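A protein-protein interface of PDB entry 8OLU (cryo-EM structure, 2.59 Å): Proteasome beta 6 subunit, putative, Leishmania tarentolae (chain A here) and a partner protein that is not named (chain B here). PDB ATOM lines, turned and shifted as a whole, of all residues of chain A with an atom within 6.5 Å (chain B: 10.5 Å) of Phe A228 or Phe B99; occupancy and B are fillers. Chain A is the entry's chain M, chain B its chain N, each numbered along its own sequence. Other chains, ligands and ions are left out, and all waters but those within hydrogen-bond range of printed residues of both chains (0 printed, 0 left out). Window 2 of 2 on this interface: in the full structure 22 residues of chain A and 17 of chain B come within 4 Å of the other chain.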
ATOM      1  N   TRP A 126     -20.877 -37.233  20.228  1.00  0.00           N
ATOM      2  CA  TRP A 126     -20.276 -35.926  20.609  1.00  0.00           C
ATOM      3  C   TRP A 126     -18.892 -35.783  19.986  1.00  0.00           C
ATOM      4  O   TRP A 126     -17.923 -36.404  20.436  1.00  0.00           O
ATOM      5  CB  TRP A 126     -20.156 -35.699  22.133  1.00  0.00           C
ATOM      6  CG  TRP A 126     -19.691 -34.296  22.470  1.00  0.00           C
ATOM      7  CD1 TRP A 126     -20.459 -33.170  22.466  1.00  0.00           C
ATOM      8  CD2 TRP A 126     -18.344 -33.842  22.737  1.00  0.00           C
ATOM      9  NE1 TRP A 126     -19.692 -32.068  22.749  1.00  0.00           N
ATOM     10  CE2 TRP A 126     -18.388 -32.445  22.872  1.00  0.00           C
ATOM     11  CE3 TRP A 126     -17.095 -34.468  22.816  1.00  0.00           C
ATOM     12  CZ2 TRP A 126     -17.259 -31.676  23.152  1.00  0.00           C
ATOM     13  CZ3 TRP A 126     -15.963 -33.716  23.067  1.00  0.00           C
ATOM     14  CH2 TRP A 126     -16.055 -32.336  23.273  1.00  0.00           C
ATOM     15  N   PRO A 128     -15.873 -32.911  19.344  1.00  0.00           N
ATOM     16  CA  PRO A 128     -15.274 -31.635  19.776  1.00  0.00           C
ATOM     17  C   PRO A 128     -15.107 -30.591  18.657  1.00  0.00           C
ATOM     18  O   PRO A 128     -14.560 -29.514  18.887  1.00  0.00           O
ATOM     19  CB  PRO A 128     -13.881 -32.049  20.259  1.00  0.00           C
ATOM     20  CG  PRO A 128     -13.548 -33.216  19.355  1.00  0.00           C
ATOM     21  CD  PRO A 128     -14.866 -33.928  19.048  1.00  0.00           C
ATOM     22  N   TYR A 129     -15.613 -30.942  17.464  1.00  0.00           N
ATOM     23  CA  TYR A 129     -15.465 -30.153  16.275  1.00  0.00           C
ATOM     24  C   TYR A 129     -16.827 -29.882  15.672  1.00  0.00           C
ATOM     25  O   TYR A 129     -17.664 -30.766  15.585  1.00  0.00           O
ATOM     26  CB  TYR A 129     -14.613 -30.896  15.251  1.00  0.00           C
ATOM     27  CG  TYR A 129     -13.157 -31.072  15.593  1.00  0.00           C
ATOM     28  CD1 TYR A 129     -12.355 -29.976  15.873  1.00  0.00           C
ATOM     29  CD2 TYR A 129     -12.548 -32.313  15.567  1.00  0.00           C
ATOM     30  CE1 TYR A 129     -11.004 -30.102  16.149  1.00  0.00           C
ATOM     31  CE2 TYR A 129     -11.192 -32.466  15.872  1.00  0.00           C
ATOM     32  CZ  TYR A 129     -10.404 -31.350  16.130  1.00  0.00           C
ATOM     33  OH  TYR A 129      -9.053 -31.436  16.403  1.00  0.00           O
ATOM     34  N   ASP A 185     -12.534 -22.530  18.018  1.00  0.00           N
ATOM     35  CA  ASP A 185     -11.108 -22.733  17.899  1.00  0.00           C
ATOM     36  C   ASP A 185     -10.465 -21.511  17.335  1.00  0.00           C
ATOM     37  O   ASP A 185      -9.346 -21.236  17.638  1.00  0.00           O
ATOM     38  CB  ASP A 185     -10.767 -23.901  16.964  1.00  0.00           C
ATOM     39  CG  ASP A 185     -10.760 -25.237  17.715  1.00  0.00           C
ATOM     40  OD1 ASP A 185     -10.754 -25.168  18.996  1.00  0.00           O
ATOM     41  OD2 ASP A 185     -10.747 -26.332  17.043  1.00  0.00           O
ATOM     42  N   HIS A 224       2.203 -27.272  16.262  1.00  0.00           N
ATOM     43  CA  HIS A 224       2.339 -27.832  17.575  1.00  0.00           C
ATOM     44  C   HIS A 224       1.066 -28.507  18.028  1.00  0.00           C
ATOM     45  O   HIS A 224       1.121 -29.262  18.960  1.00  0.00           O
ATOM     46  CB  HIS A 224       2.826 -26.782  18.547  1.00  0.00           C
ATOM     47  CG  HIS A 224       4.252 -26.380  18.270  1.00  0.00           C
ATOM     48  ND1 HIS A 224       4.857 -25.238  18.776  1.00  0.00           N
ATOM     49  CD2 HIS A 224       5.189 -26.995  17.481  1.00  0.00           C
ATOM     50  CE1 HIS A 224       6.119 -25.189  18.343  1.00  0.00           C
ATOM     51  NE2 HIS A 224       6.340 -26.258  17.520  1.00  0.00           N
ATOM     52  N   ARG A 225      -0.044 -28.351  17.341  1.00  0.00           N
ATOM     53  CA  ARG A 225      -1.256 -29.040  17.721  1.00  0.00           C
ATOM     54  C   ARG A 225      -1.671 -30.082  16.704  1.00  0.00           C
ATOM     55  O   ARG A 225      -2.718 -30.663  16.869  1.00  0.00           O
ATOM     56  CB  ARG A 225      -2.404 -28.049  17.812  1.00  0.00           C
ATOM     57  CG  ARG A 225      -2.329 -27.081  18.986  1.00  0.00           C
ATOM     58  CD  ARG A 225      -2.684 -27.665  20.357  1.00  0.00           C
ATOM     59  NE  ARG A 225      -4.053 -28.182  20.358  1.00  0.00           N
ATOM     60  CZ  ARG A 225      -5.133 -27.430  20.257  1.00  0.00           C
ATOM     61  NH1 ARG A 225      -5.213 -26.310  20.959  1.00  0.00           N
ATOM     62  NH2 ARG A 225      -6.110 -27.805  19.450  1.00  0.00           N
ATOM     63  N   ARG A 226      -0.960 -30.193  15.581  1.00  0.00           N
ATOM     64  CA  ARG A 226      -0.773 -31.416  14.811  1.00  0.00           C
ATOM     65  C   ARG A 226      -1.753 -32.493  15.275  1.00  0.00           C
ATOM     66  O   ARG A 226      -2.657 -32.861  14.535  1.00  0.00           O
ATOM     67  CB  ARG A 226       0.713 -31.781  15.022  1.00  0.00           C
ATOM     68  CG  ARG A 226       1.443 -32.592  13.957  1.00  0.00           C
ATOM     69  CD  ARG A 226       0.605 -32.775  12.702  1.00  0.00           C
ATOM     70  NE  ARG A 226       0.773 -34.149  12.256  1.00  0.00           N
ATOM     71  CZ  ARG A 226       0.627 -34.547  11.013  1.00  0.00           C
ATOM     72  NH1 ARG A 226       1.142 -35.703  10.640  1.00  0.00           N
ATOM     73  NH2 ARG A 226       0.032 -33.743  10.147  1.00  0.00           N
ATOM     74  N   PHE A 227      -1.595 -32.920  16.541  1.00  0.00           N
ATOM     75  CA  PHE A 227      -2.168 -34.144  17.079  1.00  0.00           C
ATOM     76  C   PHE A 227      -3.648 -33.974  17.434  1.00  0.00           C
ATOM     77  O   PHE A 227      -4.458 -34.780  16.968  1.00  0.00           O
ATOM     78  CB  PHE A 227      -1.230 -34.678  18.169  1.00  0.00           C
ATOM     79  CG  PHE A 227       0.113 -35.061  17.581  1.00  0.00           C
ATOM     80  CD1 PHE A 227       0.191 -35.786  16.386  1.00  0.00           C
ATOM     81  CD2 PHE A 227       1.306 -34.655  18.175  1.00  0.00           C
ATOM     82  CE1 PHE A 227       1.418 -36.093  15.802  1.00  0.00           C
ATOM     83  CE2 PHE A 227       2.536 -34.971  17.598  1.00  0.00           C
ATOM     84  CZ  PHE A 227       2.592 -35.679  16.407  1.00  0.00           C
ATOM     85  N   PHE A 228      -4.016 -32.937  18.210  1.00  0.00           N
ATOM     86  CA  PHE A 228      -5.414 -32.492  18.299  1.00  0.00           C
ATOM     87  C   PHE A 228      -5.589 -31.114  17.660  1.00  0.00           C
ATOM     88  O   PHE A 228      -5.494 -30.078  18.311  1.00  0.00           O
ATOM     89  CB  PHE A 228      -5.876 -32.442  19.759  1.00  0.00           C
ATOM     90  CG  PHE A 228      -7.292 -31.958  19.966  1.00  0.00           C
ATOM     91  CD1 PHE A 228      -8.314 -32.367  19.127  1.00  0.00           C
ATOM     92  CD2 PHE A 228      -7.597 -31.119  21.036  1.00  0.00           C
ATOM     93  CE1 PHE A 228      -9.611 -31.920  19.341  1.00  0.00           C
ATOM     94  CE2 PHE A 228      -8.895 -30.686  21.255  1.00  0.00           C
ATOM     95  CZ  PHE A 228      -9.901 -31.085  20.400  1.00  0.00           C
ATOM     96  N   PRO A 229      -5.809 -31.033  16.343  1.00  0.00           N
ATOM     97  CA  PRO A 229      -5.592 -29.787  15.633  1.00  0.00           C
ATOM     98  C   PRO A 229      -6.715 -28.822  15.907  1.00  0.00           C
ATOM     99  O   PRO A 229      -7.829 -29.288  16.151  1.00  0.00           O
ATOM    100  CB  PRO A 229      -5.561 -30.163  14.155  1.00  0.00           C
ATOM    101  CG  PRO A 229      -5.874 -31.633  14.079  1.00  0.00           C
ATOM    102  CD  PRO A 229      -6.229 -32.122  15.467  1.00  0.00           C
ATOM    103  N   TYR A 230      -6.383 -27.530  15.926  1.00  0.00           N
ATOM    104  CA  TYR A 230      -7.346 -26.465  15.752  1.00  0.00           C
ATOM    105  C   TYR A 230      -8.087 -26.669  14.458  1.00  0.00           C
ATOM    106  O   TYR A 230      -7.508 -27.029  13.460  1.00  0.00           O
ATOM    107  CB  TYR A 230      -6.653 -25.121  15.568  1.00  0.00           C
ATOM    108  CG  TYR A 230      -6.030 -24.568  16.822  1.00  0.00           C
ATOM    109  CD1 TYR A 230      -6.802 -24.175  17.871  1.00  0.00           C
ATOM    110  CD2 TYR A 230      -4.666 -24.519  17.000  1.00  0.00           C
ATOM    111  CE1 TYR A 230      -6.230 -23.655  19.024  1.00  0.00           C
ATOM    112  CE2 TYR A 230      -4.073 -24.031  18.142  1.00  0.00           C
ATOM    113  CZ  TYR A 230      -4.862 -23.522  19.146  1.00  0.00           C
ATOM    114  OH  TYR A 230      -4.331 -23.070  20.340  1.00  0.00           O
ATOM    115  N   ASP B  55     -24.105 -31.312  34.196  1.00  0.00           N
ATOM    116  CA  ASP B  55     -23.060 -30.432  33.702  1.00  0.00           C
ATOM    117  C   ASP B  55     -23.376 -29.017  34.053  1.00  0.00           C
ATOM    118  O   ASP B  55     -22.643 -28.361  34.714  1.00  0.00           O
ATOM    119  CB  ASP B  55     -22.836 -30.658  32.231  1.00  0.00           C
ATOM    120  CG  ASP B  55     -22.297 -32.091  32.007  1.00  0.00           C
ATOM    121  OD1 ASP B  55     -21.738 -32.752  32.982  1.00  0.00           O
ATOM    122  OD2 ASP B  55     -22.483 -32.634  30.859  1.00  0.00           O
ATOM    123  N   SER B  91     -14.277 -21.603  30.413  1.00  0.00           N
ATOM    124  CA  SER B  91     -14.397 -22.794  31.214  1.00  0.00           C
ATOM    125  C   SER B  91     -14.923 -23.933  30.391  1.00  0.00           C
ATOM    126  O   SER B  91     -14.416 -25.019  30.483  1.00  0.00           O
ATOM    127  CB  SER B  91     -15.278 -22.556  32.388  1.00  0.00           C
ATOM    128  OG  SER B  91     -14.825 -21.425  33.116  1.00  0.00           O
ATOM    129  N   ILE B  92     -15.953 -23.668  29.624  1.00  0.00           N
ATOM    130  CA  ILE B  92     -16.622 -24.655  28.815  1.00  0.00           C
ATOM    131  C   ILE B  92     -15.717 -25.131  27.730  1.00  0.00           C
ATOM    132  O   ILE B  92     -15.805 -26.271  27.322  1.00  0.00           O
ATOM    133  CB  ILE B  92     -17.857 -24.020  28.197  1.00  0.00           C
ATOM    134  CG1 ILE B  92     -19.017 -24.133  29.151  1.00  0.00           C
ATOM    135  CG2 ILE B  92     -18.276 -24.709  26.950  1.00  0.00           C
ATOM    136  CD1 ILE B  92     -20.121 -23.174  28.834  1.00  0.00           C
ATOM    137  N   TYR B  93     -14.925 -24.230  27.208  1.00  0.00           N
ATOM    138  CA  TYR B  93     -14.008 -24.616  26.167  1.00  0.00           C
ATOM    139  C   TYR B  93     -12.934 -25.520  26.717  1.00  0.00           C
ATOM    140  O   TYR B  93     -12.619 -26.510  26.108  1.00  0.00           O
ATOM    141  CB  TYR B  93     -13.342 -23.388  25.560  1.00  0.00           C
ATOM    142  CG  TYR B  93     -12.439 -23.701  24.404  1.00  0.00           C
ATOM    143  CD1 TYR B  93     -12.933 -24.085  23.166  1.00  0.00           C
ATOM    144  CD2 TYR B  93     -11.076 -23.685  24.569  1.00  0.00           C
ATOM    145  CE1 TYR B  93     -12.103 -24.465  22.130  1.00  0.00           C
ATOM    146  CE2 TYR B  93     -10.227 -23.972  23.516  1.00  0.00           C
ATOM    147  CZ  TYR B  93     -10.749 -24.342  22.298  1.00  0.00           C
ATOM    148  OH  TYR B  93      -9.824 -24.694  21.358  1.00  0.00           O
ATOM    149  N   GLN B  94     -12.352 -25.133  27.840  1.00  0.00           N
ATOM    150  CA  GLN B  94     -11.303 -25.931  28.436  1.00  0.00           C
ATOM    151  C   GLN B  94     -11.829 -27.342  28.620  1.00  0.00           C
ATOM    152  O   GLN B  94     -11.127 -28.283  28.327  1.00  0.00           O
ATOM    153  CB  GLN B  94     -10.812 -25.404  29.779  1.00  0.00           C
ATOM    154  CG  GLN B  94      -9.555 -26.146  30.239  1.00  0.00           C
ATOM    155  CD  GLN B  94      -8.447 -26.204  29.179  1.00  0.00           C
ATOM    156  OE1 GLN B  94      -7.850 -25.177  28.815  1.00  0.00           O
ATOM    157  NE2 GLN B  94      -8.151 -27.401  28.665  1.00  0.00           N
ATOM    158  N   LYS B  95     -13.102 -27.502  28.948  1.00  0.00           N
ATOM    159  CA  LYS B  95     -13.636 -28.836  29.138  1.00  0.00           C
ATOM    160  C   LYS B  95     -13.766 -29.616  27.846  1.00  0.00           C
ATOM    161  O   LYS B  95     -13.606 -30.783  27.866  1.00  0.00           O
ATOM    162  CB  LYS B  95     -14.973 -28.747  29.855  1.00  0.00           C
ATOM    163  CG  LYS B  95     -14.812 -28.355  31.305  1.00  0.00           C
ATOM    164  CD  LYS B  95     -16.053 -28.430  32.144  1.00  0.00           C
ATOM    165  CE  LYS B  95     -16.184 -29.801  32.786  1.00  0.00           C
ATOM    166  NZ  LYS B  95     -17.226 -30.605  32.091  1.00  0.00           N
ATOM    167  N   ARG B  96     -14.008 -28.976  26.733  1.00  0.00           N
ATOM    168  CA  ARG B  96     -14.047 -29.627  25.444  1.00  0.00           C
ATOM    169  C   ARG B  96     -12.667 -29.995  24.979  1.00  0.00           C
ATOM    170  O   ARG B  96     -12.530 -30.866  24.133  1.00  0.00           O
ATOM    171  CB  ARG B  96     -14.635 -28.651  24.445  1.00  0.00           C
ATOM    172  CG  ARG B  96     -14.569 -29.038  22.983  1.00  0.00           C
ATOM    173  CD  ARG B  96     -13.576 -28.116  22.346  1.00  0.00           C
ATOM    174  NE  ARG B  96     -13.189 -28.565  21.044  1.00  0.00           N
ATOM    175  CZ  ARG B  96     -12.099 -28.128  20.457  1.00  0.00           C
ATOM    176  NH1 ARG B  96     -11.085 -27.665  21.170  1.00  0.00           N
ATOM    177  NH2 ARG B  96     -12.070 -28.140  19.140  1.00  0.00           N
ATOM    178  N   CYS B  97     -11.654 -29.358  25.571  1.00  0.00           N
ATOM    179  CA  CYS B  97     -10.282 -29.651  25.202  1.00  0.00           C
ATOM    180  C   CYS B  97      -9.747 -30.824  25.988  1.00  0.00           C
ATOM    181  O   CYS B  97      -8.736 -31.398  25.592  1.00  0.00           O
ATOM    182  CB  CYS B  97      -9.396 -28.433  25.352  1.00  0.00           C
ATOM    183  SG  CYS B  97      -9.935 -27.128  24.217  1.00  0.00           S
ATOM    184  N   ASP B  98     -10.446 -31.168  27.069  1.00  0.00           N
ATOM    185  CA  ASP B  98     -10.087 -32.260  27.948  1.00  0.00           C
ATOM    186  C   ASP B  98     -10.959 -33.447  27.617  1.00  0.00           C
ATOM    187  O   ASP B  98     -10.963 -34.426  28.358  1.00  0.00           O
ATOM    188  CB  ASP B  98     -10.282 -31.821  29.394  1.00  0.00           C
ATOM    189  CG  ASP B  98      -9.438 -30.596  29.751  1.00  0.00           C
ATOM    190  OD1 ASP B  98      -8.594 -30.185  28.896  1.00  0.00           O
ATOM    191  OD2 ASP B  98      -9.643 -30.022  30.874  1.00  0.00           O
ATOM    192  N   PHE B  99     -11.774 -33.313  26.568  1.00  0.00           N
ATOM    193  CA  PHE B  99     -12.687 -34.380  26.198  1.00  0.00           C
ATOM    194  C   PHE B  99     -13.677 -34.666  27.332  1.00  0.00           C
ATOM    195  O   PHE B  99     -14.279 -35.737  27.406  1.00  0.00           O
ATOM    196  CB  PHE B  99     -11.854 -35.585  25.741  1.00  0.00           C
ATOM    197  CG  PHE B  99     -11.178 -35.304  24.429  1.00  0.00           C
ATOM    198  CD1 PHE B  99     -11.882 -35.459  23.233  1.00  0.00           C
ATOM    199  CD2 PHE B  99      -9.891 -34.759  24.405  1.00  0.00           C
ATOM    200  CE1 PHE B  99     -11.280 -35.138  22.025  1.00  0.00           C
ATOM    201  CE2 PHE B  99      -9.299 -34.415  23.199  1.00  0.00           C
ATOM    202  CZ  PHE B  99      -9.997 -34.609  22.014  1.00  0.00           C
ATOM    203  N   ASP B 100     -13.877 -33.678  28.193  1.00  0.00           N
ATOM    204  CA  ASP B 100     -14.789 -33.790  29.302  1.00  0.00           C
ATOM    205  C   ASP B 100     -15.870 -32.725  29.141  1.00  0.00           C
ATOM    206  O   ASP B 100     -16.131 -31.918  30.014  1.00  0.00           O
ATOM    207  CB  ASP B 100     -14.047 -33.625  30.628  1.00  0.00           C
ATOM    208  CG  ASP B 100     -14.925 -34.005  31.816  1.00  0.00           C
ATOM    209  OD1 ASP B 100     -15.582 -35.097  31.732  1.00  0.00           O
ATOM    210  OD2 ASP B 100     -14.976 -33.202  32.799  1.00  0.00           O
ATOM    211  N   PRO B 101     -16.546 -32.675  27.996  1.00  0.00           N
ATOM    212  CA  PRO B 101     -17.336 -31.499  27.664  1.00  0.00           C
ATOM    213  C   PRO B 101     -18.457 -31.206  28.630  1.00  0.00           C
ATOM    214  O   PRO B 101     -18.938 -32.124  29.271  1.00  0.00           O
ATOM    215  CB  PRO B 101     -17.897 -31.912  26.327  1.00  0.00           C
ATOM    216  CG  PRO B 101     -17.953 -33.427  26.421  1.00  0.00           C
ATOM    217  CD  PRO B 101     -16.598 -33.732  26.987  1.00  0.00           C
ATOM    218  N   CYS B 102     -18.789 -29.924  28.789  1.00  0.00           N
ATOM    219  CA  CYS B 102     -19.964 -29.540  29.542  1.00  0.00           C
ATOM    220  C   CYS B 102     -21.105 -29.593  28.549  1.00  0.00           C
ATOM    221  O   CYS B 102     -21.185 -28.691  27.707  1.00  0.00           O
ATOM    222  CB  CYS B 102     -19.797 -28.158  30.169  1.00  0.00           C
ATOM    223  SG  CYS B 102     -21.336 -27.340  30.706  1.00  0.00           S
ATOM    224  N   LEU B 103     -21.937 -30.648  28.592  1.00  0.00           N
ATOM    225  CA  LEU B 103     -22.841 -30.927  27.485  1.00  0.00           C
ATOM    226  C   LEU B 103     -24.135 -30.146  27.545  1.00  0.00           C
ATOM    227  O   LEU B 103     -25.221 -30.678  27.464  1.00  0.00           O
ATOM    228  CB  LEU B 103     -23.158 -32.406  27.496  1.00  0.00           C
ATOM    229  CG  LEU B 103     -21.986 -33.277  27.074  1.00  0.00           C
ATOM    230  CD1 LEU B 103     -22.382 -34.761  27.172  1.00  0.00           C
ATOM    231  CD2 LEU B 103     -21.543 -32.893  25.664  1.00  0.00           C
ATOM    232  N   ASP B 123     -21.659 -26.440  23.896  1.00  0.00           N
ATOM    233  CA  ASP B 123     -20.804 -27.427  24.538  1.00  0.00           C
ATOM    234  C   ASP B 123     -19.370 -27.284  24.062  1.00  0.00           C
ATOM    235  O   ASP B 123     -18.455 -27.309  24.878  1.00  0.00           O
ATOM    236  CB  ASP B 123     -21.320 -28.846  24.329  1.00  0.00           C
ATOM    237  CG  ASP B 123     -21.956 -29.094  22.949  1.00  0.00           C
ATOM    238  OD1 ASP B 123     -22.966 -28.344  22.570  1.00  0.00           O
ATOM    239  OD2 ASP B 123     -21.420 -29.995  22.201  1.00  0.00           O
ATOM    240  N   VAL B 124     -19.169 -27.088  22.778  1.00  0.00           N
ATOM    241  CA  VAL B 124     -17.821 -26.966  22.272  1.00  0.00           C
ATOM    242  C   VAL B 124     -17.187 -25.610  22.489  1.00  0.00           C
ATOM    243  O   VAL B 124     -16.014 -25.522  22.189  1.00  0.00           O
ATOM    244  CB  VAL B 124     -17.745 -27.289  20.775  1.00  0.00           C
ATOM    245  CG1 VAL B 124     -18.189 -28.723  20.510  1.00  0.00           C
ATOM    246  CG2 VAL B 124     -18.561 -26.329  19.938  1.00  0.00           C
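The indole nitrogen of Trp A126 sits at hydrogen-bond distance from the side-chain carboxylate of Asp B123, at 2.8 Å.
The guanidinium group of Arg B96 sits at hydrogen-bond distance from the backbone carbonyl oxygen of Pro A128 (2.7 Å).
The side-chain hydroxyl (OH) of Tyr B93 sits at hydrogen-bond distance from the side-chain carboxylate (OD1) of Asp A185 (2.6 Å).
OD2 of Asp A185 lies within salt-bridge range of NH2 of Arg B96 (3.1 Å).
The side-chain hydroxyl of Tyr A129 lies within hydrogen-bond range of the backbone carbonyl oxygen of Pro A229 (2.5 Å).
The guanidinium group of Arg A225 lies within hydrogen-bond range of the backbone carbonyl oxygen of Phe A228 (2.6 Å).
The side-chain carboxylate of Asp B55 lies within hydrogen-bond range of the backbone NH of Leu B103, 3.1 Å away.
OH of Tyr B93 sits at hydrogen-bond distance from NH1 of Arg B96, 3.2 Å away.
The backbone carbonyl oxygen (O) of Tyr B93 lies close to the side-chain sulfur (SG) of Cys B97, 3.3 Å away.
NH1 of Arg B96 sits at hydrogen-bond distance from SG of Cys B97 (3.3 Å).
Among the printed residues, merely in contact across the chains: Trp A126 with Pro B101, Trp A126 with Leu B103, Trp A126 with Arg B96, Phe A228 with Arg B96, Tyr A129 with Arg B96, Phe A228 with Phe B99 and Pro A128 with Phe B99.
Of the printed residues of chain A, Phe B99 touches Pro A128 (3.996 Å) and Phe A228 (3.8 Å).
No residue of chain B comes within 4 Å of Pro A229.
Printed residues of chain A within 4 Å of Pro B101: Trp A126.
Printed residues of chain A within 4 Å of Arg B96: Trp A126 (3.6 Å), Pro A128 (2.7 Å), Tyr A129 (3.7 Å), Asp A185 (3.1 Å) and Phe A228 (3.7 Å).
Ser B91 touches none of the printed residues of chain A.
Val B124 touches none of the printed residues of chain A.
The nearest residue of chain B that does not touch Phe A228 is Cys B97 (4.3 Å).
The nearest printed residue of chain A that does not touch Phe B99 is Trp A126 (4.4 Å).
Of the 11 printed residues of chain A, 5 touch a printed residue of chain B.
Hydrophobic or aromatic side chains of chain A that line the printed part of chain B: Trp A126, Pro A128, Tyr A129 and Phe A228.
Among the printed residues, 11 pairs touch across the chains.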
